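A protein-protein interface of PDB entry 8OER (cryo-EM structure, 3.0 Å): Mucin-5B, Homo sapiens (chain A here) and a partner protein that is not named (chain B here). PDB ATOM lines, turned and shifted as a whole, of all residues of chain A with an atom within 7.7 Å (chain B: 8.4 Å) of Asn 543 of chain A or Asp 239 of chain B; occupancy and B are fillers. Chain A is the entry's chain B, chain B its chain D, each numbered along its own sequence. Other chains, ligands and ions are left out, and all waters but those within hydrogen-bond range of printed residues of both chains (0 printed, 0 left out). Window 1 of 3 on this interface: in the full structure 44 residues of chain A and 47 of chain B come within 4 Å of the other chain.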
ATOM      1  N   THR A 410     -21.438   8.778  11.633  1.00  0.00           N
ATOM      2  CA  THR A 410     -22.620   8.885  12.472  1.00  0.00           C
ATOM      3  C   THR A 410     -23.106  10.331  12.500  1.00  0.00           C
ATOM      4  O   THR A 410     -22.580  11.205  11.809  1.00  0.00           O
ATOM      5  CB  THR A 410     -22.325   8.375  13.875  1.00  0.00           C
ATOM      6  OG1 THR A 410     -21.642   9.386  14.615  1.00  0.00           O
ATOM      7  CG2 THR A 410     -21.445   7.159  13.812  1.00  0.00           C
ATOM      8  N   TYR A 411     -24.137  10.593  13.306  1.00  0.00           N
ATOM      9  CA  TYR A 411     -24.628  11.954  13.483  1.00  0.00           C
ATOM     10  C   TYR A 411     -23.625  12.817  14.228  1.00  0.00           C
ATOM     11  O   TYR A 411     -23.540  14.023  13.982  1.00  0.00           O
ATOM     12  CB  TYR A 411     -25.952  11.941  14.238  1.00  0.00           C
ATOM     13  CG  TYR A 411     -27.103  11.338  13.478  1.00  0.00           C
ATOM     14  CD1 TYR A 411     -27.450  11.801  12.222  1.00  0.00           C
ATOM     15  CD2 TYR A 411     -27.844  10.307  14.020  1.00  0.00           C
ATOM     16  CE1 TYR A 411     -28.499  11.252  11.534  1.00  0.00           C
ATOM     17  CE2 TYR A 411     -28.889   9.755  13.337  1.00  0.00           C
ATOM     18  CZ  TYR A 411     -29.211  10.228  12.094  1.00  0.00           C
ATOM     19  OH  TYR A 411     -30.259   9.671  11.413  1.00  0.00           O
ATOM     20  N   ASP A 412     -22.873  12.224  15.146  1.00  0.00           N
ATOM     21  CA  ASP A 412     -21.824  12.913  15.876  1.00  0.00           C
ATOM     22  C   ASP A 412     -20.515  12.973  15.097  1.00  0.00           C
ATOM     23  O   ASP A 412     -19.493  13.368  15.660  1.00  0.00           O
ATOM     24  CB  ASP A 412     -21.592  12.226  17.220  1.00  0.00           C
ATOM     25  CG  ASP A 412     -22.813  12.260  18.115  1.00  0.00           C
ATOM     26  OD1 ASP A 412     -23.695  11.404  17.944  1.00  0.00           O
ATOM     27  OD2 ASP A 412     -22.882  13.116  19.012  1.00  0.00           O
ATOM     28  N   GLU A 413     -20.529  12.579  13.825  1.00  0.00           N
ATOM     29  CA  GLU A 413     -19.341  12.574  12.972  1.00  0.00           C
ATOM     30  C   GLU A 413     -18.246  11.674  13.535  1.00  0.00           C
ATOM     31  O   GLU A 413     -17.083  12.062  13.611  1.00  0.00           O
ATOM     32  CB  GLU A 413     -18.815  13.991  12.745  1.00  0.00           C
ATOM     33  CG  GLU A 413     -19.882  15.006  12.402  1.00  0.00           C
ATOM     34  CD  GLU A 413     -20.203  15.034  10.921  1.00  0.00           C
ATOM     35  OE1 GLU A 413     -19.317  14.679  10.119  1.00  0.00           O
ATOM     36  OE2 GLU A 413     -21.335  15.413  10.557  1.00  0.00           O
ATOM     37  N   LYS A 414     -18.618  10.459  13.923  1.00  0.00           N
ATOM     38  CA  LYS A 414     -17.654   9.462  14.384  1.00  0.00           C
ATOM     39  C   LYS A 414     -17.479   8.431  13.282  1.00  0.00           C
ATOM     40  O   LYS A 414     -18.185   7.428  13.224  1.00  0.00           O
ATOM     41  CB  LYS A 414     -18.123   8.811  15.676  1.00  0.00           C
ATOM     42  CG  LYS A 414     -17.198   7.740  16.194  1.00  0.00           C
ATOM     43  CD  LYS A 414     -17.638   7.279  17.554  1.00  0.00           C
ATOM     44  CE  LYS A 414     -16.541   6.509  18.234  1.00  0.00           C
ATOM     45  NZ  LYS A 414     -16.709   6.520  19.703  1.00  0.00           N
ATOM     46  N   GLY A 538     -25.828   6.429  16.008  1.00  0.00           N
ATOM     47  CA  GLY A 538     -25.587   7.148  17.238  1.00  0.00           C
ATOM     48  C   GLY A 538     -26.725   8.077  17.608  1.00  0.00           C
ATOM     49  O   GLY A 538     -27.626   8.366  16.824  1.00  0.00           O
ATOM     50  N   ASN A 539     -26.656   8.580  18.839  1.00  0.00           N
ATOM     51  CA  ASN A 539     -27.791   9.236  19.468  1.00  0.00           C
ATOM     52  C   ASN A 539     -27.905  10.714  19.141  1.00  0.00           C
ATOM     53  O   ASN A 539     -28.813  11.367  19.659  1.00  0.00           O
ATOM     54  CB  ASN A 539     -27.730   9.057  20.985  1.00  0.00           C
ATOM     55  CG  ASN A 539     -26.406   9.470  21.568  1.00  0.00           C
ATOM     56  OD1 ASN A 539     -25.544  10.008  20.877  1.00  0.00           O
ATOM     57  ND2 ASN A 539     -26.230   9.214  22.854  1.00  0.00           N
ATOM     58  N   PHE A 540     -27.012  11.264  18.325  1.00  0.00           N
ATOM     59  CA  PHE A 540     -27.150  12.633  17.849  1.00  0.00           C
ATOM     60  C   PHE A 540     -27.250  13.611  19.020  1.00  0.00           C
ATOM     61  O   PHE A 540     -28.266  14.271  19.223  1.00  0.00           O
ATOM     62  CB  PHE A 540     -28.368  12.741  16.929  1.00  0.00           C
ATOM     63  CG  PHE A 540     -28.438  14.009  16.140  1.00  0.00           C
ATOM     64  CD1 PHE A 540     -27.317  14.768  15.912  1.00  0.00           C
ATOM     65  CD2 PHE A 540     -29.637  14.424  15.606  1.00  0.00           C
ATOM     66  CE1 PHE A 540     -27.399  15.913  15.180  1.00  0.00           C
ATOM     67  CE2 PHE A 540     -29.718  15.567  14.874  1.00  0.00           C
ATOM     68  CZ  PHE A 540     -28.603  16.314  14.665  1.00  0.00           C
ATOM     69  N   ASN A 541     -26.175  13.678  19.812  1.00  0.00           N
ATOM     70  CA  ASN A 541     -26.147  14.550  20.980  1.00  0.00           C
ATOM     71  C   ASN A 541     -24.866  15.368  21.058  1.00  0.00           C
ATOM     72  O   ASN A 541     -24.520  15.859  22.135  1.00  0.00           O
ATOM     73  CB  ASN A 541     -26.327  13.746  22.267  1.00  0.00           C
ATOM     74  CG  ASN A 541     -25.112  12.922  22.609  1.00  0.00           C
ATOM     75  OD1 ASN A 541     -24.359  12.505  21.730  1.00  0.00           O
ATOM     76  ND2 ASN A 541     -24.919  12.666  23.894  1.00  0.00           N
ATOM     77  N   GLN A 542     -24.158  15.517  19.943  1.00  0.00           N
ATOM     78  CA  GLN A 542     -22.922  16.293  19.869  1.00  0.00           C
ATOM     79  C   GLN A 542     -21.911  15.813  20.911  1.00  0.00           C
ATOM     80  O   GLN A 542     -21.466  16.547  21.792  1.00  0.00           O
ATOM     81  CB  GLN A 542     -23.218  17.785  20.004  1.00  0.00           C
ATOM     82  CG  GLN A 542     -24.421  18.205  19.205  1.00  0.00           C
ATOM     83  CD  GLN A 542     -24.426  17.605  17.819  1.00  0.00           C
ATOM     84  OE1 GLN A 542     -23.404  17.569  17.135  1.00  0.00           O
ATOM     85  NE2 GLN A 542     -25.578  17.110  17.402  1.00  0.00           N
ATOM     86  N   ASN A 543     -21.570  14.536  20.789  1.00  0.00           N
ATOM     87  CA  ASN A 543     -20.623  13.875  21.678  1.00  0.00           C
ATOM     88  C   ASN A 543     -20.164  12.623  20.952  1.00  0.00           C
ATOM     89  O   ASN A 543     -20.982  11.741  20.678  1.00  0.00           O
ATOM     90  CB  ASN A 543     -21.287  13.539  23.011  1.00  0.00           C
ATOM     91  CG  ASN A 543     -20.391  12.755  23.937  1.00  0.00           C
ATOM     92  OD1 ASN A 543     -19.215  12.546  23.659  1.00  0.00           O
ATOM     93  ND2 ASN A 543     -20.952  12.309  25.052  1.00  0.00           N
ATOM     94  N   GLN A 544     -18.882  12.553  20.615  1.00  0.00           N
ATOM     95  CA  GLN A 544     -18.370  11.415  19.867  1.00  0.00           C
ATOM     96  C   GLN A 544     -18.028  10.228  20.746  1.00  0.00           C
ATOM     97  O   GLN A 544     -17.840   9.128  20.224  1.00  0.00           O
ATOM     98  CB  GLN A 544     -17.135  11.825  19.082  1.00  0.00           C
ATOM     99  CG  GLN A 544     -17.442  12.699  17.908  1.00  0.00           C
ATOM    100  CD  GLN A 544     -16.288  12.775  16.947  1.00  0.00           C
ATOM    101  OE1 GLN A 544     -16.392  13.372  15.880  1.00  0.00           O
ATOM    102  NE2 GLN A 544     -15.168  12.174  17.324  1.00  0.00           N
ATOM    103  N   ALA A 545     -17.932  10.418  22.052  1.00  0.00           N
ATOM    104  CA  ALA A 545     -17.566   9.333  22.943  1.00  0.00           C
ATOM    105  C   ALA A 545     -18.754   8.494  23.377  1.00  0.00           C
ATOM    106  O   ALA A 545     -18.556   7.370  23.846  1.00  0.00           O
ATOM    107  CB  ALA A 545     -16.860   9.883  24.180  1.00  0.00           C
ATOM    108  N   ASP A 546     -19.972   9.002  23.236  1.00  0.00           N
ATOM    109  CA  ASP A 546     -21.159   8.291  23.678  1.00  0.00           C
ATOM    110  C   ASP A 546     -21.792   7.461  22.580  1.00  0.00           C
ATOM    111  O   ASP A 546     -22.778   6.770  22.839  1.00  0.00           O
ATOM    112  CB  ASP A 546     -22.190   9.277  24.242  1.00  0.00           C
ATOM    113  CG  ASP A 546     -23.104   9.870  23.175  1.00  0.00           C
ATOM    114  OD1 ASP A 546     -22.699  10.014  22.003  1.00  0.00           O
ATOM    115  OD2 ASP A 546     -24.249  10.210  23.526  1.00  0.00           O
ATOM    116  N   ASP A 547     -21.258   7.515  21.362  1.00  0.00           N
ATOM    117  CA  ASP A 547     -21.942   6.900  20.236  1.00  0.00           C
ATOM    118  C   ASP A 547     -22.063   5.398  20.409  1.00  0.00           C
ATOM    119  O   ASP A 547     -23.077   4.808  20.027  1.00  0.00           O
ATOM    120  CB  ASP A 547     -21.208   7.221  18.944  1.00  0.00           C
ATOM    121  CG  ASP A 547     -21.853   8.337  18.194  1.00  0.00           C
ATOM    122  OD1 ASP A 547     -22.511   9.165  18.853  1.00  0.00           O
ATOM    123  OD2 ASP A 547     -21.710   8.390  16.959  1.00  0.00           O
ATOM    124  N   PHE A 548     -21.053   4.764  20.991  1.00  0.00           N
ATOM    125  CA  PHE A 548     -21.049   3.324  21.165  1.00  0.00           C
ATOM    126  C   PHE A 548     -21.811   2.892  22.406  1.00  0.00           C
ATOM    127  O   PHE A 548     -21.612   1.775  22.891  1.00  0.00           O
ATOM    128  CB  PHE A 548     -19.612   2.811  21.215  1.00  0.00           C
ATOM    129  CG  PHE A 548     -18.943   2.780  19.883  1.00  0.00           C
ATOM    130  CD1 PHE A 548     -19.607   3.203  18.757  1.00  0.00           C
ATOM    131  CD2 PHE A 548     -17.648   2.352  19.757  1.00  0.00           C
ATOM    132  CE1 PHE A 548     -18.999   3.185  17.539  1.00  0.00           C
ATOM    133  CE2 PHE A 548     -17.039   2.336  18.536  1.00  0.00           C
ATOM    134  CZ  PHE A 548     -17.717   2.752  17.426  1.00  0.00           C
ATOM    135  N   THR A 549     -22.671   3.752  22.934  1.00  0.00           N
ATOM    136  CA  THR A 549     -23.523   3.366  24.045  1.00  0.00           C
ATOM    137  C   THR A 549     -24.566   2.378  23.549  1.00  0.00           C
ATOM    138  O   THR A 549     -25.545   2.771  22.908  1.00  0.00           O
ATOM    139  CB  THR A 549     -24.201   4.593  24.643  1.00  0.00           C
ATOM    140  OG1 THR A 549     -23.261   5.669  24.716  1.00  0.00           O
ATOM    141  CG2 THR A 549     -24.712   4.292  26.030  1.00  0.00           C
ATOM    142  N   VAL A 555     -20.468   2.061  26.801  1.00  0.00           N
ATOM    143  CA  VAL A 555     -19.856   2.327  25.508  1.00  0.00           C
ATOM    144  C   VAL A 555     -19.078   1.100  25.056  1.00  0.00           C
ATOM    145  O   VAL A 555     -18.234   0.575  25.791  1.00  0.00           O
ATOM    146  CB  VAL A 555     -18.942   3.553  25.608  1.00  0.00           C
ATOM    147  CG1 VAL A 555     -18.155   3.737  24.332  1.00  0.00           C
ATOM    148  CG2 VAL A 555     -19.751   4.787  25.943  1.00  0.00           C
ATOM    149  N   CYS B  99     -15.002   9.917  36.527  1.00  0.00           N
ATOM    150  CA  CYS B  99     -13.796   9.404  35.893  1.00  0.00           C
ATOM    151  C   CYS B  99     -12.921  10.549  35.402  1.00  0.00           C
ATOM    152  O   CYS B  99     -13.406  11.490  34.769  1.00  0.00           O
ATOM    153  CB  CYS B  99     -14.140   8.475  34.732  1.00  0.00           C
ATOM    154  SG  CYS B  99     -14.918   6.917  35.211  1.00  0.00           S
ATOM    155  N   GLY B 101     -10.884  12.813  33.335  1.00  0.00           N
ATOM    156  CA  GLY B 101     -10.723  13.037  31.908  1.00  0.00           C
ATOM    157  C   GLY B 101      -9.262  13.054  31.510  1.00  0.00           C
ATOM    158  O   GLY B 101      -8.386  13.347  32.313  1.00  0.00           O
ATOM    159  N   THR B 113      -7.587  14.910  22.345  1.00  0.00           N
ATOM    160  CA  THR B 113      -8.092  15.954  23.217  1.00  0.00           C
ATOM    161  C   THR B 113      -8.852  15.344  24.388  1.00  0.00           C
ATOM    162  O   THR B 113      -8.981  14.127  24.521  1.00  0.00           O
ATOM    163  CB  THR B 113      -8.986  16.904  22.437  1.00  0.00           C
ATOM    164  OG1 THR B 113     -10.172  16.216  22.041  1.00  0.00           O
ATOM    165  CG2 THR B 113      -8.276  17.358  21.191  1.00  0.00           C
ATOM    166  N   PHE B 114      -9.363  16.214  25.257  1.00  0.00           N
ATOM    167  CA  PHE B 114     -10.064  15.744  26.445  1.00  0.00           C
ATOM    168  C   PHE B 114     -11.365  15.049  26.078  1.00  0.00           C
ATOM    169  O   PHE B 114     -11.823  14.150  26.793  1.00  0.00           O
ATOM    170  CB  PHE B 114     -10.345  16.916  27.383  1.00  0.00           C
ATOM    171  CG  PHE B 114      -9.220  17.240  28.322  1.00  0.00           C
ATOM    172  CD1 PHE B 114      -8.862  16.365  29.321  1.00  0.00           C
ATOM    173  CD2 PHE B 114      -8.548  18.438  28.224  1.00  0.00           C
ATOM    174  CE1 PHE B 114      -7.851  16.679  30.182  1.00  0.00           C
ATOM    175  CE2 PHE B 114      -7.536  18.746  29.083  1.00  0.00           C
ATOM    176  CZ  PHE B 114      -7.187  17.871  30.057  1.00  0.00           C
ATOM    177  N   ASP B 115     -11.980  15.464  24.973  1.00  0.00           N
ATOM    178  CA  ASP B 115     -13.282  14.980  24.537  1.00  0.00           C
ATOM    179  C   ASP B 115     -13.192  13.761  23.638  1.00  0.00           C
ATOM    180  O   ASP B 115     -14.216  13.344  23.092  1.00  0.00           O
ATOM    181  CB  ASP B 115     -14.038  16.087  23.803  1.00  0.00           C
ATOM    182  CG  ASP B 115     -14.317  17.283  24.682  1.00  0.00           C
ATOM    183  OD1 ASP B 115     -14.787  17.102  25.822  1.00  0.00           O
ATOM    184  OD2 ASP B 115     -14.050  18.410  24.232  1.00  0.00           O
ATOM    185  N   GLY B 116     -12.001  13.197  23.457  1.00  0.00           N
ATOM    186  CA  GLY B 116     -11.824  12.021  22.640  1.00  0.00           C
ATOM    187  C   GLY B 116     -11.424  12.282  21.207  1.00  0.00           C
ATOM    188  O   GLY B 116     -11.240  11.320  20.455  1.00  0.00           O
ATOM    189  N   GLN B 224     -13.400  16.189  37.184  1.00  0.00           N
ATOM    190  CA  GLN B 224     -14.599  16.629  36.485  1.00  0.00           C
ATOM    191  C   GLN B 224     -14.963  18.074  36.793  1.00  0.00           C
ATOM    192  O   GLN B 224     -15.858  18.620  36.143  1.00  0.00           O
ATOM    193  CB  GLN B 224     -15.767  15.713  36.834  1.00  0.00           C
ATOM    194  CG  GLN B 224     -15.512  14.247  36.539  1.00  0.00           C
ATOM    195  CD  GLN B 224     -16.265  13.757  35.320  1.00  0.00           C
ATOM    196  OE1 GLN B 224     -16.949  14.526  34.652  1.00  0.00           O
ATOM    197  NE2 GLN B 224     -16.149  12.468  35.032  1.00  0.00           N
ATOM    198  N   LYS B 227     -14.374  20.803  33.909  1.00  0.00           N
ATOM    199  CA  LYS B 227     -15.065  20.538  32.659  1.00  0.00           C
ATOM    200  C   LYS B 227     -15.564  21.836  32.042  1.00  0.00           C
ATOM    201  O   LYS B 227     -16.106  22.697  32.736  1.00  0.00           O
ATOM    202  CB  LYS B 227     -16.223  19.581  32.909  1.00  0.00           C
ATOM    203  CG  LYS B 227     -16.976  19.177  31.672  1.00  0.00           C
ATOM    204  CD  LYS B 227     -16.692  17.738  31.310  1.00  0.00           C
ATOM    205  CE  LYS B 227     -17.751  16.807  31.861  1.00  0.00           C
ATOM    206  NZ  LYS B 227     -17.360  15.383  31.688  1.00  0.00           N
ATOM    207  N   GLY B 228     -15.364  21.983  30.735  1.00  0.00           N
ATOM    208  CA  GLY B 228     -15.865  23.124  30.008  1.00  0.00           C
ATOM    209  C   GLY B 228     -15.099  24.410  30.204  1.00  0.00           C
ATOM    210  O   GLY B 228     -15.259  25.332  29.395  1.00  0.00           O
ATOM    211  N   GLY B 235      -8.400  20.641  23.747  1.00  0.00           N
ATOM    212  CA  GLY B 235      -9.808  20.934  23.662  1.00  0.00           C
ATOM    213  C   GLY B 235     -10.262  21.681  24.896  1.00  0.00           C
ATOM    214  O   GLY B 235      -9.477  22.046  25.765  1.00  0.00           O
ATOM    215  N   ASN B 236     -11.571  21.903  24.963  1.00  0.00           N
ATOM    216  CA  ASN B 236     -12.164  22.612  26.085  1.00  0.00           C
ATOM    217  C   ASN B 236     -12.889  21.687  27.048  1.00  0.00           C
ATOM    218  O   ASN B 236     -13.592  22.171  27.936  1.00  0.00           O
ATOM    219  CB  ASN B 236     -13.107  23.706  25.587  1.00  0.00           C
ATOM    220  CG  ASN B 236     -14.362  23.157  24.967  1.00  0.00           C
ATOM    221  OD1 ASN B 236     -14.346  22.105  24.336  1.00  0.00           O
ATOM    222  ND2 ASN B 236     -15.463  23.872  25.134  1.00  0.00           N
ATOM    223  N   PHE B 237     -12.732  20.377  26.902  1.00  0.00           N
ATOM    224  CA  PHE B 237     -13.294  19.415  27.840  1.00  0.00           C
ATOM    225  C   PHE B 237     -14.783  19.670  28.042  1.00  0.00           C
ATOM    226  O   PHE B 237     -15.241  20.015  29.128  1.00  0.00           O
ATOM    227  CB  PHE B 237     -12.534  19.466  29.164  1.00  0.00           C
ATOM    228  CG  PHE B 237     -12.793  18.301  30.073  1.00  0.00           C
ATOM    229  CD1 PHE B 237     -13.500  17.207  29.645  1.00  0.00           C
ATOM    230  CD2 PHE B 237     -12.293  18.296  31.359  1.00  0.00           C
ATOM    231  CE1 PHE B 237     -13.719  16.143  30.490  1.00  0.00           C
ATOM    232  CE2 PHE B 237     -12.511  17.236  32.202  1.00  0.00           C
ATOM    233  CZ  PHE B 237     -13.221  16.160  31.767  1.00  0.00           C
ATOM    234  N   ASP B 238     -15.539  19.523  26.957  1.00  0.00           N
ATOM    235  CA  ASP B 238     -16.973  19.777  26.991  1.00  0.00           C
ATOM    236  C   ASP B 238     -17.794  18.579  26.539  1.00  0.00           C
ATOM    237  O   ASP B 238     -19.000  18.725  26.310  1.00  0.00           O
ATOM    238  CB  ASP B 238     -17.322  20.994  26.132  1.00  0.00           C
ATOM    239  CG  ASP B 238     -16.985  20.794  24.668  1.00  0.00           C
ATOM    240  OD1 ASP B 238     -16.273  19.827  24.345  1.00  0.00           O
ATOM    241  OD2 ASP B 238     -17.431  21.607  23.836  1.00  0.00           O
ATOM    242  N   ASP B 239     -17.181  17.400  26.417  1.00  0.00           N
ATOM    243  CA  ASP B 239     -17.855  16.205  25.910  1.00  0.00           C
ATOM    244  C   ASP B 239     -18.458  16.463  24.534  1.00  0.00           C
ATOM    245  O   ASP B 239     -19.526  15.955  24.194  1.00  0.00           O
ATOM    246  CB  ASP B 239     -18.922  15.709  26.884  1.00  0.00           C
ATOM    247  CG  ASP B 239     -18.503  15.845  28.329  1.00  0.00           C
ATOM    248  OD1 ASP B 239     -18.387  16.986  28.811  1.00  0.00           O
ATOM    249  OD2 ASP B 239     -18.290  14.809  28.990  1.00  0.00           O
ATOM    250  N   ASN B 240     -17.766  17.269  23.736  1.00  0.00           N
ATOM    251  CA  ASN B 240     -18.232  17.636  22.399  1.00  0.00           C
ATOM    252  C   ASN B 240     -16.981  17.825  21.544  1.00  0.00           C
ATOM    253  O   ASN B 240     -16.379  18.900  21.533  1.00  0.00           O
ATOM    254  CB  ASN B 240     -19.088  18.892  22.437  1.00  0.00           C
ATOM    255  CG  ASN B 240     -19.556  19.324  21.067  1.00  0.00           C
ATOM    256  OD1 ASN B 240     -19.137  18.783  20.048  1.00  0.00           O
ATOM    257  ND2 ASN B 240     -20.438  20.311  21.036  1.00  0.00           N
ATOM    258  N   ALA B 241     -16.611  16.774  20.823  1.00  0.00           N
ATOM    259  CA  ALA B 241     -15.342  16.755  20.116  1.00  0.00           C
ATOM    260  C   ALA B 241     -15.392  17.451  18.765  1.00  0.00           C
ATOM    261  O   ALA B 241     -14.338  17.653  18.155  1.00  0.00           O
ATOM    262  CB  ALA B 241     -14.875  15.313  19.931  1.00  0.00           C
ATOM    263  N   ILE B 242     -16.574  17.811  18.275  1.00  0.00           N
ATOM    264  CA  ILE B 242     -16.647  18.429  16.956  1.00  0.00           C
ATOM    265  C   ILE B 242     -16.132  19.860  17.005  1.00  0.00           C
ATOM    266  O   ILE B 242     -15.519  20.344  16.049  1.00  0.00           O
ATOM    267  CB  ILE B 242     -18.082  18.360  16.414  1.00  0.00           C
ATOM    268  CG1 ILE B 242     -18.832  17.188  17.048  1.00  0.00           C
ATOM    269  CG2 ILE B 242     -18.062  18.222  14.902  1.00  0.00           C
ATOM    270  CD1 ILE B 242     -20.305  17.163  16.722  1.00  0.00           C
ATOM    271  N   ASN B 243     -16.381  20.560  18.108  1.00  0.00           N
ATOM    272  CA  ASN B 243     -16.014  21.961  18.255  1.00  0.00           C
ATOM    273  C   ASN B 243     -14.698  22.153  18.992  1.00  0.00           C
ATOM    274  O   ASN B 243     -14.341  23.290  19.309  1.00  0.00           O
ATOM    275  CB  ASN B 243     -17.124  22.721  18.976  1.00  0.00           C
ATOM    276  CG  ASN B 243     -16.955  22.707  20.477  1.00  0.00           C
ATOM    277  OD1 ASN B 243     -16.702  21.667  21.076  1.00  0.00           O
ATOM    278  ND2 ASN B 243     -17.083  23.873  21.092  1.00  0.00           N
ATOM    279  N   ASP B 244     -13.971  21.074  19.279  1.00  0.00           N
ATOM    280  CA  ASP B 244     -12.717  21.200  20.006  1.00  0.00           C
ATOM    281  C   ASP B 244     -11.644  21.919  19.210  1.00  0.00           C
ATOM    282  O   ASP B 244     -10.647  22.344  19.796  1.00  0.00           O
ATOM    283  CB  ASP B 244     -12.209  19.827  20.424  1.00  0.00           C
ATOM    284  CG  ASP B 244     -12.400  19.574  21.891  1.00  0.00           C
ATOM    285  OD1 ASP B 244     -13.173  20.328  22.510  1.00  0.00           O
ATOM    286  OD2 ASP B 244     -11.789  18.631  22.426  1.00  0.00           O
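The side-chain amide oxygen (OD1) of Asn 543 of chain A lies close to the backbone carbonyl oxygen (O) of Asp 239 of chain B. O of Gln 542 of chain A lies close to O of Asp 239 of chain B, 3.1 Å away.
OD2 of Asp 412 of chain A lies close to N of Gln 542 of chain A (2.9 Å). OD1 of Asn 543 of chain A sits at hydrogen-bond distance from N of Ala 545 of chain A, 3.0 Å away. The side-chain carboxylate of Asp 115 of chain B is in hydrogen-bond range of the backbone NH of Asp 239 of chain B (2.5 Å). NZ of Lys 227 of chain B lies within salt-bridge range of OD2 of Asp 239 of chain B. The backbone NH (N) of Ile 242 of chain B lies within hydrogen-bond range of the side-chain amide oxygen (OD1) of Asn 240 of chain B.
Among the printed residues, merely in contact across the chains: Gln 542 of chain A with Ile 242 of chain B (3.2 Å) and Gln 542 of chain A with Asn 240 of chain B (3.4 Å).
Of the printed residues of chain B, Gln 542 of chain A touches Asp 239 (3.1 Å), Asn 240 (3.4 Å) and Ile 242 (3.2 Å). Of chain B, only Asp 239 (3.2 Å) comes within 4 Å of Asn 543 of chain A. Gly 116 of chain B touches none of the printed residues of chain A. Printed residues of chain A within 4 Å of Asp 239 of chain B: Gln 542 and Asn 543. Of the printed residues of chain A, Asn 240 of chain B touches Gln 542 (3.4 Å). Of the printed residues of chain A, Ile 242 of chain B touches Gln 542 (3.2 Å). The nearest printed residue of chain B that does not touch Gln 542 of chain A is Ala 241 of chain B (5.0 Å).
Hydrophobic or aromatic side chains of chain B within 4 Å of the printed part of chain A: Ile 242. Of the 18 printed residues of chain A, 2 touch a printed residue of chain B. Among the printed residues, 4 pairs touch across the chains.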
